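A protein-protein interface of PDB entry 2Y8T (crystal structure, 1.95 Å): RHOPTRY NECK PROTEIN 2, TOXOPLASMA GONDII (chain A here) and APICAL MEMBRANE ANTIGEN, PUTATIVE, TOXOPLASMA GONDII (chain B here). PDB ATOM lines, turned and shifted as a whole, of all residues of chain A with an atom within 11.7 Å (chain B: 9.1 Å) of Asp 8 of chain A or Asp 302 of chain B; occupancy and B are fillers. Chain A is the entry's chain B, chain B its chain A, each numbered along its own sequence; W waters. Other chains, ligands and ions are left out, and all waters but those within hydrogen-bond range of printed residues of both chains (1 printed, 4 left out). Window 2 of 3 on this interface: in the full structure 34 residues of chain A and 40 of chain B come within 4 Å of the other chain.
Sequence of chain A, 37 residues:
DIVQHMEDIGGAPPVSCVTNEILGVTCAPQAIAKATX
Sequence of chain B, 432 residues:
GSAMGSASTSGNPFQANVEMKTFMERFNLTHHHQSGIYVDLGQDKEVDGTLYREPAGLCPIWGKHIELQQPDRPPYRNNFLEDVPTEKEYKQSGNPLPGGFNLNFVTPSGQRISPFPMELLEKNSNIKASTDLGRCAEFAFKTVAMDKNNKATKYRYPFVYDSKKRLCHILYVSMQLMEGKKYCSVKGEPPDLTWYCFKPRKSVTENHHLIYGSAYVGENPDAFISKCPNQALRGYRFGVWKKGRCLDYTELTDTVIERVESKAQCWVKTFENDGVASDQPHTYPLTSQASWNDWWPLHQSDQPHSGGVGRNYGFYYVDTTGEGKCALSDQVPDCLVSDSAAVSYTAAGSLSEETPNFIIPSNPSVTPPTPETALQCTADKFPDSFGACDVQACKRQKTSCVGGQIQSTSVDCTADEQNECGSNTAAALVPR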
ATOM      1  N   ASP A   1      17.491 -34.522  18.780  1.00  0.00           N
ATOM      2  CA  ASP A   1      18.569 -35.384  18.223  1.00  0.00           C
ATOM      3  C   ASP A   1      19.352 -34.528  17.215  1.00  0.00           C
ATOM      4  O   ASP A   1      19.130 -33.325  17.116  1.00  0.00           O
ATOM      5  CB  ASP A   1      17.959 -36.631  17.544  1.00  0.00           C
ATOM      6  CG  ASP A   1      17.107 -36.291  16.262  1.00  0.00           C
ATOM      7  OD1 ASP A   1      16.599 -35.151  16.089  1.00  0.00           O
ATOM      8  OD2 ASP A   1      16.940 -37.179  15.392  1.00  0.00           O
ATOM      9  N   ILE A   2      20.226 -35.157  16.440  1.00  0.00           N
ATOM     10  CA  ILE A   2      21.015 -34.440  15.469  1.00  0.00           C
ATOM     11  C   ILE A   2      20.174 -33.829  14.330  1.00  0.00           C
ATOM     12  O   ILE A   2      20.509 -32.753  13.821  1.00  0.00           O
ATOM     13  CB  ILE A   2      22.138 -35.302  14.909  1.00  0.00           C
ATOM     14  CG1 ILE A   2      23.095 -34.408  14.098  1.00  0.00           C
ATOM     15  CG2 ILE A   2      21.569 -36.480  14.081  1.00  0.00           C
ATOM     16  CD1 ILE A   2      23.841 -33.372  14.899  1.00  0.00           C
ATOM     17  N   VAL A   3      19.106 -34.503  13.915  1.00  0.00           N
ATOM     18  CA  VAL A   3      18.239 -33.896  12.894  1.00  0.00           C
ATOM     19  C   VAL A   3      17.528 -32.643  13.369  1.00  0.00           C
ATOM     20  O   VAL A   3      17.627 -31.630  12.710  1.00  0.00           O
ATOM     21  CB  VAL A   3      17.391 -34.874  12.009  1.00  0.00           C
ATOM     22  CG1 VAL A   3      17.458 -36.285  12.433  1.00  0.00           C
ATOM     23  CG2 VAL A   3      16.039 -34.373  11.568  1.00  0.00           C
ATOM     24  N   GLN A   4      16.959 -32.663  14.560  1.00  0.00           N
ATOM     25  CA  GLN A   4      16.363 -31.444  15.051  1.00  0.00           C
ATOM     26  C   GLN A   4      17.435 -30.345  15.200  1.00  0.00           C
ATOM     27  O   GLN A   4      17.221 -29.190  14.789  1.00  0.00           O
ATOM     28  CB  GLN A   4      15.595 -31.641  16.357  1.00  0.00           C
ATOM     29  CG  GLN A   4      14.728 -30.377  16.740  1.00  0.00           C
ATOM     30  CD  GLN A   4      13.682 -30.048  15.652  1.00  0.00           C
ATOM     31  OE1 GLN A   4      12.813 -30.879  15.344  1.00  0.00           O
ATOM     32  NE2 GLN A   4      13.788 -28.868  15.043  1.00  0.00           N
ATOM     33  N   HIS A   5      18.578 -30.682  15.767  1.00  0.00           N
ATOM     34  CA  HIS A   5      19.620 -29.624  15.942  1.00  0.00           C
ATOM     35  C   HIS A   5      20.002 -28.983  14.588  1.00  0.00           C
ATOM     36  O   HIS A   5      20.070 -27.758  14.477  1.00  0.00           O
ATOM     37  CB  HIS A   5      20.875 -30.182  16.524  1.00  0.00           C
ATOM     38  CG  HIS A   5      21.945 -29.157  16.660  1.00  0.00           C
ATOM     39  ND1 HIS A   5      21.880 -28.156  17.606  1.00  0.00           N
ATOM     40  CD2 HIS A   5      23.070 -28.932  15.943  1.00  0.00           C
ATOM     41  CE1 HIS A   5      22.933 -27.370  17.479  1.00  0.00           C
ATOM     42  NE2 HIS A   5      23.670 -27.817  16.479  1.00  0.00           N
ATOM     43  N   MET A   6      20.327 -29.814  13.590  1.00  0.00           N
ATOM     44  CA  MET A   6      20.663 -29.303  12.257  1.00  0.00           C
ATOM     45  C   MET A   6      19.536 -28.470  11.688  1.00  0.00           C
ATOM     46  O   MET A   6      19.798 -27.401  11.150  1.00  0.00           O
ATOM     47  CB  MET A   6      21.063 -30.443  11.286  1.00  0.00           C
ATOM     48  CG  MET A   6      22.393 -31.147  11.714  1.00  0.00           C
ATOM     49  SD  MET A   6      23.801 -30.025  11.908  1.00  0.00           S
ATOM     50  CE  MET A   6      24.111 -29.889  10.121  1.00  0.00           C
ATOM     51  N   GLU A   7      18.276 -28.906  11.851  1.00  0.00           N
ATOM     52  CA  GLU A   7      17.136 -28.124  11.283  1.00  0.00           C
ATOM     53  C   GLU A   7      17.035 -26.743  11.959  1.00  0.00           C
ATOM     54  O   GLU A   7      16.823 -25.747  11.297  1.00  0.00           O
ATOM     55  CB  GLU A   7      15.813 -28.901  11.430  1.00  0.00           C
ATOM     56  CG  GLU A   7      14.650 -28.417  10.530  1.00  0.00           C
ATOM     57  CD  GLU A   7      13.743 -27.374  11.197  1.00  0.00           C
ATOM     58  OE1 GLU A   7      13.647 -27.381  12.442  1.00  0.00           O
ATOM     59  OE2 GLU A   7      13.095 -26.578  10.474  1.00  0.00           O
ATOM     60  N   ASP A   8      17.248 -26.701  13.276  1.00  0.00           N
ATOM     61  CA  ASP A   8      17.144 -25.453  14.019  1.00  0.00           C
ATOM     62  C   ASP A   8      18.216 -24.458  13.541  1.00  0.00           C
ATOM     63  O   ASP A   8      18.017 -23.290  13.668  1.00  0.00           O
ATOM     64  CB  ASP A   8      17.398 -25.678  15.514  1.00  0.00           C
ATOM     65  CG  ASP A   8      16.302 -26.481  16.218  1.00  0.00           C
ATOM     66  OD1 ASP A   8      15.177 -26.627  15.703  1.00  0.00           O
ATOM     67  OD2 ASP A   8      16.638 -26.996  17.319  1.00  0.00           O
ATOM     68  N   ILE A   9      19.355 -24.912  13.006  1.00  0.00           N
ATOM     69  CA  ILE A   9      20.349 -23.911  12.548  1.00  0.00           C
ATOM     70  C   ILE A   9      20.368 -23.709  11.012  1.00  0.00           C
ATOM     71  O   ILE A   9      21.290 -23.091  10.456  1.00  0.00           O
ATOM     72  CB  ILE A   9      21.760 -24.231  13.075  1.00  0.00           C
ATOM     73  CG1 ILE A   9      22.280 -25.558  12.464  1.00  0.00           C
ATOM     74  CG2 ILE A   9      21.759 -24.266  14.667  1.00  0.00           C
ATOM     75  CD1 ILE A   9      23.837 -25.852  12.761  1.00  0.00           C
ATOM     76  N   GLY A  10      19.325 -24.146  10.330  1.00  0.00           N
ATOM     77  CA  GLY A  10      19.192 -23.879   8.909  1.00  0.00           C
ATOM     78  C   GLY A  10      19.622 -25.040   8.000  1.00  0.00           C
ATOM     79  O   GLY A  10      19.768 -24.866   6.799  1.00  0.00           O
ATOM     80  N   GLY A  11      19.834 -26.220   8.555  1.00  0.00           N
ATOM     81  CA  GLY A  11      20.180 -27.433   7.743  1.00  0.00           C
ATOM     82  C   GLY A  11      19.124 -27.607   6.628  1.00  0.00           C
ATOM     83  O   GLY A  11      17.952 -27.535   6.885  1.00  0.00           O
ATOM     84  N   ALA A  12      19.541 -27.752   5.370  1.00  0.00           N
ATOM     85  CA  ALA A  12      18.591 -27.679   4.250  1.00  0.00           C
ATOM     86  C   ALA A  12      18.060 -29.059   3.771  1.00  0.00           C
ATOM     87  O   ALA A  12      18.584 -30.090   4.134  1.00  0.00           O
ATOM     88  CB  ALA A  12      19.219 -26.884   3.101  1.00  0.00           C
ATOM     89  N   PRO A  13      16.911 -29.092   3.081  1.00  0.00           N
ATOM     90  CA  PRO A  13      16.436 -30.413   2.646  1.00  0.00           C
ATOM     91  C   PRO A  13      17.477 -31.208   1.813  1.00  0.00           C
ATOM     92  O   PRO A  13      18.337 -30.633   1.145  1.00  0.00           O
ATOM     93  CB  PRO A  13      15.182 -30.104   1.789  1.00  0.00           C
ATOM     94  CG  PRO A  13      15.186 -28.596   1.542  1.00  0.00           C
ATOM     95  CD  PRO A  13      16.146 -27.949   2.528  1.00  0.00           C
ATOM     96  N   9AT A  37      23.775 -32.493   2.956  1.00  0.00           N
ATOM     97  CA  9AT A  37      22.551 -33.304   2.819  1.00  0.00           C
ATOM     98  C   9AT A  37      22.575 -34.009   1.447  1.00  0.00           C
ATOM     99  O   9AT A  37      22.593 -33.398   0.374  1.00  0.00           O
ATOM    100  CB  9AT A  37      21.348 -32.418   3.074  1.00  0.00           C
ATOM    101  OG1 9AT A  37      21.531 -31.272   2.269  1.00  0.00           O
ATOM    102  CG2 9AT A  37      21.357 -31.993   4.540  1.00  0.00           C
ATOM    103  NXT 9AT A  37      22.869 -35.296   1.532  1.00  0.00           N
ATOM    104  N   VAL B  39      22.363 -13.802  11.393  1.00  0.00           N
ATOM    105  CA  VAL B  39      21.756 -15.057  10.875  1.00  0.00           C
ATOM    106  C   VAL B  39      20.290 -14.773  10.452  1.00  0.00           C
ATOM    107  O   VAL B  39      19.444 -14.310  11.285  1.00  0.00           O
ATOM    108  CB  VAL B  39      21.799 -16.215  11.957  1.00  0.00           C
ATOM    109  CG1 VAL B  39      21.066 -17.514  11.424  1.00  0.00           C
ATOM    110  CG2 VAL B  39      23.252 -16.568  12.240  1.00  0.00           C
ATOM    111  N   ASP B  40      20.011 -15.015   9.167  1.00  0.00           N
ATOM    112  CA  ASP B  40      18.672 -14.895   8.575  1.00  0.00           C
ATOM    113  C   ASP B  40      18.077 -16.292   8.316  1.00  0.00           C
ATOM    114  O   ASP B  40      18.495 -17.033   7.354  1.00  0.00           O
ATOM    115  CB  ASP B  40      18.744 -14.106   7.267  1.00  0.00           C
ATOM    116  CG  ASP B  40      17.393 -13.939   6.614  1.00  0.00           C
ATOM    117  OD1 ASP B  40      16.340 -14.463   7.103  1.00  0.00           O
ATOM    118  OD2 ASP B  40      17.395 -13.205   5.628  1.00  0.00           O
ATOM    119  N   LEU B  41      17.094 -16.641   9.163  1.00  0.00           N
ATOM    120  CA  LEU B  41      16.333 -17.904   9.005  1.00  0.00           C
ATOM    121  C   LEU B  41      14.885 -17.557   9.327  1.00  0.00           C
ATOM    122  O   LEU B  41      14.253 -18.182  10.152  1.00  0.00           O
ATOM    123  CB  LEU B  41      16.892 -18.954   9.990  1.00  0.00           C
ATOM    124  CG  LEU B  41      18.311 -19.431   9.593  1.00  0.00           C
ATOM    125  CD1 LEU B  41      18.921 -20.379  10.666  1.00  0.00           C
ATOM    126  CD2 LEU B  41      18.325 -20.140   8.156  1.00  0.00           C
ATOM    127  N   GLN B  43      11.915 -17.748   7.865  1.00  0.00           N
ATOM    128  CA  GLN B  43      10.745 -18.402   7.244  1.00  0.00           C
ATOM    129  C   GLN B  43      10.890 -19.893   7.424  1.00  0.00           C
ATOM    130  O   GLN B  43      11.969 -20.345   7.796  1.00  0.00           O
ATOM    131  CB  GLN B  43      10.666 -18.056   5.738  1.00  0.00           C
ATOM    132  CG  GLN B  43       9.809 -16.851   5.523  1.00  0.00           C
ATOM    133  CD  GLN B  43       9.850 -16.330   4.124  1.00  0.00           C
ATOM    134  OE1 GLN B  43      10.427 -16.927   3.185  1.00  0.00           O
ATOM    135  NE2 GLN B  43       9.271 -15.175   3.969  1.00  0.00           N
ATOM    136  N   ASP B  44       9.782 -20.630   7.293  1.00  0.00           N
ATOM    137  CA  ASP B  44       9.785 -22.083   7.369  1.00  0.00           C
ATOM    138  C   ASP B  44       9.079 -22.603   6.142  1.00  0.00           C
ATOM    139  O   ASP B  44       8.076 -21.999   5.698  1.00  0.00           O
ATOM    140  CB  ASP B  44       9.053 -22.576   8.632  1.00  0.00           C
ATOM    141  CG  ASP B  44       9.731 -22.102   9.903  1.00  0.00           C
ATOM    142  OD1 ASP B  44      10.911 -22.465  10.107  1.00  0.00           O
ATOM    143  OD2 ASP B  44       9.151 -21.258  10.626  1.00  0.00           O
ATOM    144  N   LEU B  51       9.523 -29.697   7.704  1.00  0.00           N
ATOM    145  CA  LEU B  51       9.636 -28.250   7.723  1.00  0.00           C
ATOM    146  C   LEU B  51      11.111 -27.855   7.853  1.00  0.00           C
ATOM    147  O   LEU B  51      11.847 -28.435   8.660  1.00  0.00           O
ATOM    148  CB  LEU B  51       8.852 -27.755   8.932  1.00  0.00           C
ATOM    149  CG  LEU B  51       7.860 -26.603   8.853  1.00  0.00           C
ATOM    150  CD1 LEU B  51       6.477 -27.075   9.275  1.00  0.00           C
ATOM    151  CD2 LEU B  51       8.366 -25.648   9.925  1.00  0.00           C
ATOM    152  N   TYR B  52      11.562 -26.902   7.041  1.00  0.00           N
ATOM    153  CA  TYR B  52      12.911 -26.399   7.099  1.00  0.00           C
ATOM    154  C   TYR B  52      12.910 -24.876   7.274  1.00  0.00           C
ATOM    155  O   TYR B  52      12.019 -24.183   6.757  1.00  0.00           O
ATOM    156  CB  TYR B  52      13.629 -26.709   5.783  1.00  0.00           C
ATOM    157  CG  TYR B  52      13.811 -28.203   5.563  1.00  0.00           C
ATOM    158  CD1 TYR B  52      14.946 -28.857   6.050  1.00  0.00           C
ATOM    159  CD2 TYR B  52      12.849 -28.946   4.864  1.00  0.00           C
ATOM    160  CE1 TYR B  52      15.117 -30.257   5.866  1.00  0.00           C
ATOM    161  CE2 TYR B  52      12.980 -30.325   4.702  1.00  0.00           C
ATOM    162  CZ  TYR B  52      14.147 -30.962   5.159  1.00  0.00           C
ATOM    163  OH  TYR B  52      14.304 -32.322   4.975  1.00  0.00           O
ATOM    164  N   ARG B  53      13.939 -24.372   7.942  1.00  0.00           N
ATOM    165  CA  ARG B  53      14.113 -22.941   8.104  1.00  0.00           C
ATOM    166  C   ARG B  53      14.673 -22.328   6.799  1.00  0.00           C
ATOM    167  O   ARG B  53      15.556 -22.917   6.139  1.00  0.00           O
ATOM    168  CB  ARG B  53      15.110 -22.678   9.243  1.00  0.00           C
ATOM    169  CG  ARG B  53      14.622 -23.263  10.570  1.00  0.00           C
ATOM    170  CD  ARG B  53      15.337 -22.640  11.799  1.00  0.00           C
ATOM    171  NE  ARG B  53      14.842 -21.261  11.983  1.00  0.00           N
ATOM    172  CZ  ARG B  53      15.318 -20.423  12.900  1.00  0.00           C
ATOM    173  NH1 ARG B  53      16.396 -20.788  13.603  1.00  0.00           N
ATOM    174  NH2 ARG B  53      14.806 -19.186  13.023  1.00  0.00           N
ATOM    175  N   GLU B  54      14.265 -21.098   6.498  1.00  0.00           N
ATOM    176  CA  GLU B  54      14.619 -20.518   5.229  1.00  0.00           C
ATOM    177  C   GLU B  54      15.029 -19.049   5.425  1.00  0.00           C
ATOM    178  O   GLU B  54      14.286 -18.302   6.062  1.00  0.00           O
ATOM    179  CB  GLU B  54      13.404 -20.598   4.296  1.00  0.00           C
ATOM    180  CG  GLU B  54      13.712 -20.156   2.872  1.00  0.00           C
ATOM    181  CD  GLU B  54      12.437 -19.965   2.079  1.00  0.00           C
ATOM    182  OE1 GLU B  54      11.409 -19.513   2.652  1.00  0.00           O
ATOM    183  OE2 GLU B  54      12.471 -20.203   0.867  1.00  0.00           O
ATOM    184  N   SER B 174      22.229 -23.136   3.517  1.00  0.00           N
ATOM    185  CA  SER B 174      21.546 -22.009   4.104  1.00  0.00           C
ATOM    186  C   SER B 174      21.929 -21.786   5.587  1.00  0.00           C
ATOM    187  O   SER B 174      21.648 -20.728   6.120  1.00  0.00           O
ATOM    188  CB  SER B 174      20.035 -22.264   4.024  1.00  0.00           C
ATOM    189  OG  SER B 174      19.681 -22.359   2.666  1.00  0.00           O
ATOM    190  N   MET B 175      22.660 -22.726   6.199  1.00  0.00           N
ATOM    191  CA  MET B 175      23.209 -22.487   7.538  1.00  0.00           C
ATOM    192  C   MET B 175      24.184 -21.309   7.483  1.00  0.00           C
ATOM    193  O   MET B 175      24.931 -21.168   6.501  1.00  0.00           O
ATOM    194  CB  MET B 175      23.970 -23.718   8.032  1.00  0.00           C
ATOM    195  CG  MET B 175      23.054 -24.892   8.340  1.00  0.00           C
ATOM    196  SD  MET B 175      23.964 -26.323   8.960  1.00  0.00           S
ATOM    197  CE  MET B 175      24.973 -26.801   7.554  1.00  0.00           C
ATOM    198  N   GLN B 176      24.269 -20.542   8.573  1.00  0.00           N
ATOM    199  CA  GLN B 176      25.144 -19.352   8.594  1.00  0.00           C
ATOM    200  C   GLN B 176      26.043 -19.377   9.819  1.00  0.00           C
ATOM    201  O   GLN B 176      27.109 -18.750   9.832  1.00  0.00           O
ATOM    202  CB  GLN B 176      24.246 -18.076   8.626  1.00  0.00           C
ATOM    203  CG  GLN B 176      23.617 -17.911   7.242  1.00  0.00           C
ATOM    204  CD  GLN B 176      22.288 -17.195   7.347  1.00  0.00           C
ATOM    205  OE1 GLN B 176      22.244 -15.993   7.612  1.00  0.00           O
ATOM    206  NE2 GLN B 176      21.204 -17.937   7.162  1.00  0.00           N
ATOM    207  N   LEU B 177      25.669 -20.200  10.787  1.00  0.00           N
ATOM    208  CA  LEU B 177      26.435 -20.275  12.038  1.00  0.00           C
ATOM    209  C   LEU B 177      26.486 -21.681  12.604  1.00  0.00           C
ATOM    210  O   LEU B 177      25.472 -22.268  12.992  1.00  0.00           O
ATOM    211  CB  LEU B 177      25.891 -19.295  13.083  1.00  0.00           C
ATOM    212  CG  LEU B 177      26.495 -19.298  14.506  1.00  0.00           C
ATOM    213  CD1 LEU B 177      27.830 -18.779  14.460  1.00  0.00           C
ATOM    214  CD2 LEU B 177      25.661 -18.281  15.330  1.00  0.00           C
ATOM    215  N   TYR B 183      29.613 -30.489  17.854  1.00  0.00           N
ATOM    216  CA  TYR B 183      29.191 -30.554  16.424  1.00  0.00           C
ATOM    217  C   TYR B 183      30.192 -30.207  15.335  1.00  0.00           C
ATOM    218  O   TYR B 183      30.001 -30.604  14.190  1.00  0.00           O
ATOM    219  CB  TYR B 183      27.955 -29.709  16.182  1.00  0.00           C
ATOM    220  CG  TYR B 183      26.843 -29.974  17.158  1.00  0.00           C
ATOM    221  CD1 TYR B 183      25.953 -31.003  16.957  1.00  0.00           C
ATOM    222  CD2 TYR B 183      26.656 -29.145  18.256  1.00  0.00           C
ATOM    223  CE1 TYR B 183      24.895 -31.249  17.866  1.00  0.00           C
ATOM    224  CE2 TYR B 183      25.622 -29.361  19.152  1.00  0.00           C
ATOM    225  CZ  TYR B 183      24.723 -30.396  18.934  1.00  0.00           C
ATOM    226  OH  TYR B 183      23.698 -30.592  19.832  1.00  0.00           O
ATOM    227  N   SER B 278      19.158 -11.482  14.944  1.00  0.00           N
ATOM    228  CA  SER B 278      19.643 -12.737  14.499  1.00  0.00           C
ATOM    229  C   SER B 278      18.589 -13.773  14.736  1.00  0.00           C
ATOM    230  O   SER B 278      17.898 -13.689  15.761  1.00  0.00           O
ATOM    231  CB  SER B 278      20.892 -13.093  15.304  1.00  0.00           C
ATOM    232  OG  SER B 278      21.286 -14.419  15.019  1.00  0.00           O
ATOM    233  N   ASP B 279      18.512 -14.798  13.866  1.00  0.00           N
ATOM    234  CA  ASP B 279      17.461 -15.838  13.995  1.00  0.00           C
ATOM    235  C   ASP B 279      18.035 -17.170  14.538  1.00  0.00           C
ATOM    236  O   ASP B 279      17.415 -18.239  14.453  1.00  0.00           O
ATOM    237  CB  ASP B 279      16.757 -16.022  12.629  1.00  0.00           C
ATOM    238  CG  ASP B 279      15.994 -14.787  12.205  1.00  0.00           C
ATOM    239  OD1 ASP B 279      15.716 -13.878  13.064  1.00  0.00           O
ATOM    240  OD2 ASP B 279      15.787 -14.617  10.982  1.00  0.00           O
ATOM    241  N   GLN B 280      19.296 -17.131  14.968  1.00  0.00           N
ATOM    242  CA  GLN B 280      20.013 -18.343  15.386  1.00  0.00           C
ATOM    243  C   GLN B 280      19.515 -18.782  16.798  1.00  0.00           C
ATOM    244  O   GLN B 280      19.368 -17.937  17.697  1.00  0.00           O
ATOM    245  CB  GLN B 280      21.529 -18.091  15.411  1.00  0.00           C
ATOM    246  CG  GLN B 280      22.353 -19.314  15.888  1.00  0.00           C
ATOM    247  CD  GLN B 280      22.693 -20.289  14.748  1.00  0.00           C
ATOM    248  OE1 GLN B 280      23.510 -21.215  14.923  1.00  0.00           O
ATOM    249  NE2 GLN B 280      22.153 -20.035  13.578  1.00  0.00           N
ATOM    250  N   PRO B 281      19.295 -20.111  17.015  1.00  0.00           N
ATOM    251  CA  PRO B 281      18.835 -20.616  18.330  1.00  0.00           C
ATOM    252  C   PRO B 281      19.683 -20.074  19.472  1.00  0.00           C
ATOM    253  O   PRO B 281      20.881 -19.871  19.237  1.00  0.00           O
ATOM    254  CB  PRO B 281      19.053 -22.144  18.214  1.00  0.00           C
ATOM    255  CG  PRO B 281      18.908 -22.446  16.771  1.00  0.00           C
ATOM    256  CD  PRO B 281      19.282 -21.186  15.985  1.00  0.00           C
ATOM    257  N   ASP B 302      14.578 -24.472  19.614  1.00  0.00           N
ATOM    258  CA  ASP B 302      14.466 -23.008  19.656  1.00  0.00           C
ATOM    259  C   ASP B 302      14.703 -22.385  18.279  1.00  0.00           C
ATOM    260  O   ASP B 302      15.749 -22.603  17.688  1.00  0.00           O
ATOM    261  CB  ASP B 302      15.502 -22.473  20.612  1.00  0.00           C
ATOM    262  CG  ASP B 302      15.394 -21.001  20.783  1.00  0.00           C
ATOM    263  OD1 ASP B 302      14.245 -20.537  20.997  1.00  0.00           O
ATOM    264  OD2 ASP B 302      16.440 -20.327  20.723  1.00  0.00           O
ATOM    265  N   GLN B 303      13.746 -21.611  17.769  1.00  0.00           N
ATOM    266  CA  GLN B 303      13.887 -21.019  16.422  1.00  0.00           C
ATOM    267  C   GLN B 303      13.410 -19.569  16.424  1.00  0.00           C
ATOM    268  O   GLN B 303      12.290 -19.274  16.067  1.00  0.00           O
ATOM    269  CB  GLN B 303      13.120 -21.855  15.385  1.00  0.00           C
ATOM    270  CG  GLN B 303      13.657 -23.297  15.285  1.00  0.00           C
ATOM    271  CD  GLN B 303      13.028 -24.077  14.159  1.00  0.00           C
ATOM    272  OE1 GLN B 303      12.166 -23.556  13.440  1.00  0.00           O
ATOM    273  NE2 GLN B 303      13.509 -25.327  13.945  1.00  0.00           N
ATOM    274  N   PRO B 304      14.243 -18.667  16.926  1.00  0.00           N
ATOM    275  CA  PRO B 304      13.815 -17.289  17.071  1.00  0.00           C
ATOM    276  C   PRO B 304      13.598 -16.637  15.717  1.00  0.00           C
ATOM    277  O   PRO B 304      14.308 -16.951  14.745  1.00  0.00           O
ATOM    278  CB  PRO B 304      15.006 -16.621  17.779  1.00  0.00           C
ATOM    279  CG  PRO B 304      15.916 -17.722  18.177  1.00  0.00           C
ATOM    280  CD  PRO B 304      15.638 -18.886  17.345  1.00  0.00           C
ATOM    281  N   HIS B 305      12.605 -15.759  15.638  1.00  0.00           N
ATOM    282  CA  HIS B 305      12.388 -14.954  14.450  1.00  0.00           C
ATOM    283  C   HIS B 305      12.573 -13.521  14.962  1.00  0.00           C
ATOM    284  O   HIS B 305      11.713 -12.978  15.649  1.00  0.00           O
ATOM    285  CB  HIS B 305      10.985 -15.183  13.860  1.00  0.00           C
ATOM    286  CG  HIS B 305      10.864 -16.449  13.065  1.00  0.00           C
ATOM    287  ND1 HIS B 305       9.718 -16.796  12.384  1.00  0.00           N
ATOM    288  CD2 HIS B 305      11.774 -17.414  12.781  1.00  0.00           C
ATOM    289  CE1 HIS B 305       9.900 -17.958  11.781  1.00  0.00           C
ATOM    290  NE2 HIS B 305      11.124 -18.379  12.054  1.00  0.00           N
HETATM  291  O   HOH W   1      16.278 -25.843   8.579  1.00  0.00           O
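NH1 of Arg 53 of chain B is in hydrogen-bond range of O of Asp 8 of chain A (3.0 Å).
The backbone NH (N) of Arg 53 of chain B sits at hydrogen-bond distance from the side-chain carboxylate (OE2) of Glu 7 of chain A (3.5 Å).
NE2 of Gln 303 of chain B sits at hydrogen-bond distance from OE1 of Glu 7 of chain A, at 2.5 Å.
The side-chain carboxylate of Glu 7 of chain A sits close to the backbone carbonyl oxygen of Leu 51 of chain B.
NE2 of Gln 303 of chain B lies within hydrogen-bond range of OD1 of Asp 8 of chain A.
O of Asp 279 of chain B sits at hydrogen-bond distance from NH1 of Arg 53 of chain B (2.9 Å).
NE2 of Gln 4 of chain A lies within hydrogen-bond range of OE1 of Glu 7 of chain A (3.0 Å).
The backbone carbonyl oxygen (O) of Ser 174 of chain B is in hydrogen-bond range of the side-chain amide nitrogen (NE2) of Gln 176 of chain B.
The backbone carbonyl oxygen (O) of Pro 13 of chain A is in hydrogen-bond range of OG1 of 9AT 37 of chain A, 3.4 Å away.
The side-chain carboxylate (OD2) of Asp 279 of chain B is in hydrogen-bond range of the backbone NH (N) of Leu 41 of chain B, at 3.0 Å.
The backbone carbonyl oxygen of Leu 177 of chain B lies close to the side-chain amide oxygen of Gln 280 of chain B, 2.9 Å away.
Among the printed residues, merely in contact across the chains: Ile 2 of chain A with Tyr 183 of chain B, Gln 4 of chain A with Gln 303 of chain B, His 5 of chain A with Tyr 183 of chain B, Met 6 of chain A with Met 175 of chain B, Glu 7 of chain A with Tyr 52 of chain B, Asp 8 of chain A with Pro 281 of chain B, Asp 8 of chain A with Asp 302 of chain B, Ile 9 of chain A with Leu 41 of chain B, Ile 9 of chain A with Met 175 of chain B, Ile 9 of chain A with Leu 177 of chain B, Ile 9 of chain A with Gln 280 of chain B, Ile 9 of chain A with Pro 281 of chain B, Gly 10 of chain A with Leu 41 of chain B, Gly 10 of chain A with Ser 174 of chain B, Gly 10 of chain A with Met 175 of chain B, Gly 11 of chain A with Tyr 52 of chain B, Gly 11 of chain A with Met 175 of chain B, Ala 12 of chain A with Tyr 52 of chain B and Pro 13 of chain A with Tyr 52 of chain B.
Of the printed residues of chain B, Asp 8 of chain A touches Arg 53 (3.0 Å), Pro 281 (3.3 Å), Asp 302 (3.99 Å) and Gln 303 (2.8 Å).
Of the printed residues of chain A, Tyr 183 of chain B touches Ile 2 and His 5.
Ser 278 of chain B touches none of the printed residues of chain A.
Of the printed residues of chain A, Pro 281 of chain B touches Asp 8 (3.3 Å) and Ile 9 (3.98 Å).
Printed residues of chain A within 4 Å of Asp 302 of chain B: Asp 8 (3.99 Å).
Gln 303 of chain B touches three residues of chain A.
No residue of chain A comes within 4 Å of Pro 304 of chain B.
The nearest printed residue of chain B that does not touch Asp 8 of chain A is Leu 41 of chain B (4.3 Å).
The nearest printed residue of chain A that does not touch Asp 302 of chain B is Ile 9 of chain A (6.3 Å).
The nearest printed residue of chain A that does not touch Leu 177 of chain B is His 5 of chain A (6.8 Å).
Of the 22 printed residues of chain B, 12 touch a printed residue of chain A.
Among the printed residues, 24 pairs touch across the chains.
Water W1 lies within hydrogen-bond range of the backbone carbonyl oxygen (O) of Glu 7 of chain A, the backbone NH (N) of Arg 53 of chain B and the backbone carbonyl oxygen (O) of Gly 11 of chain A.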
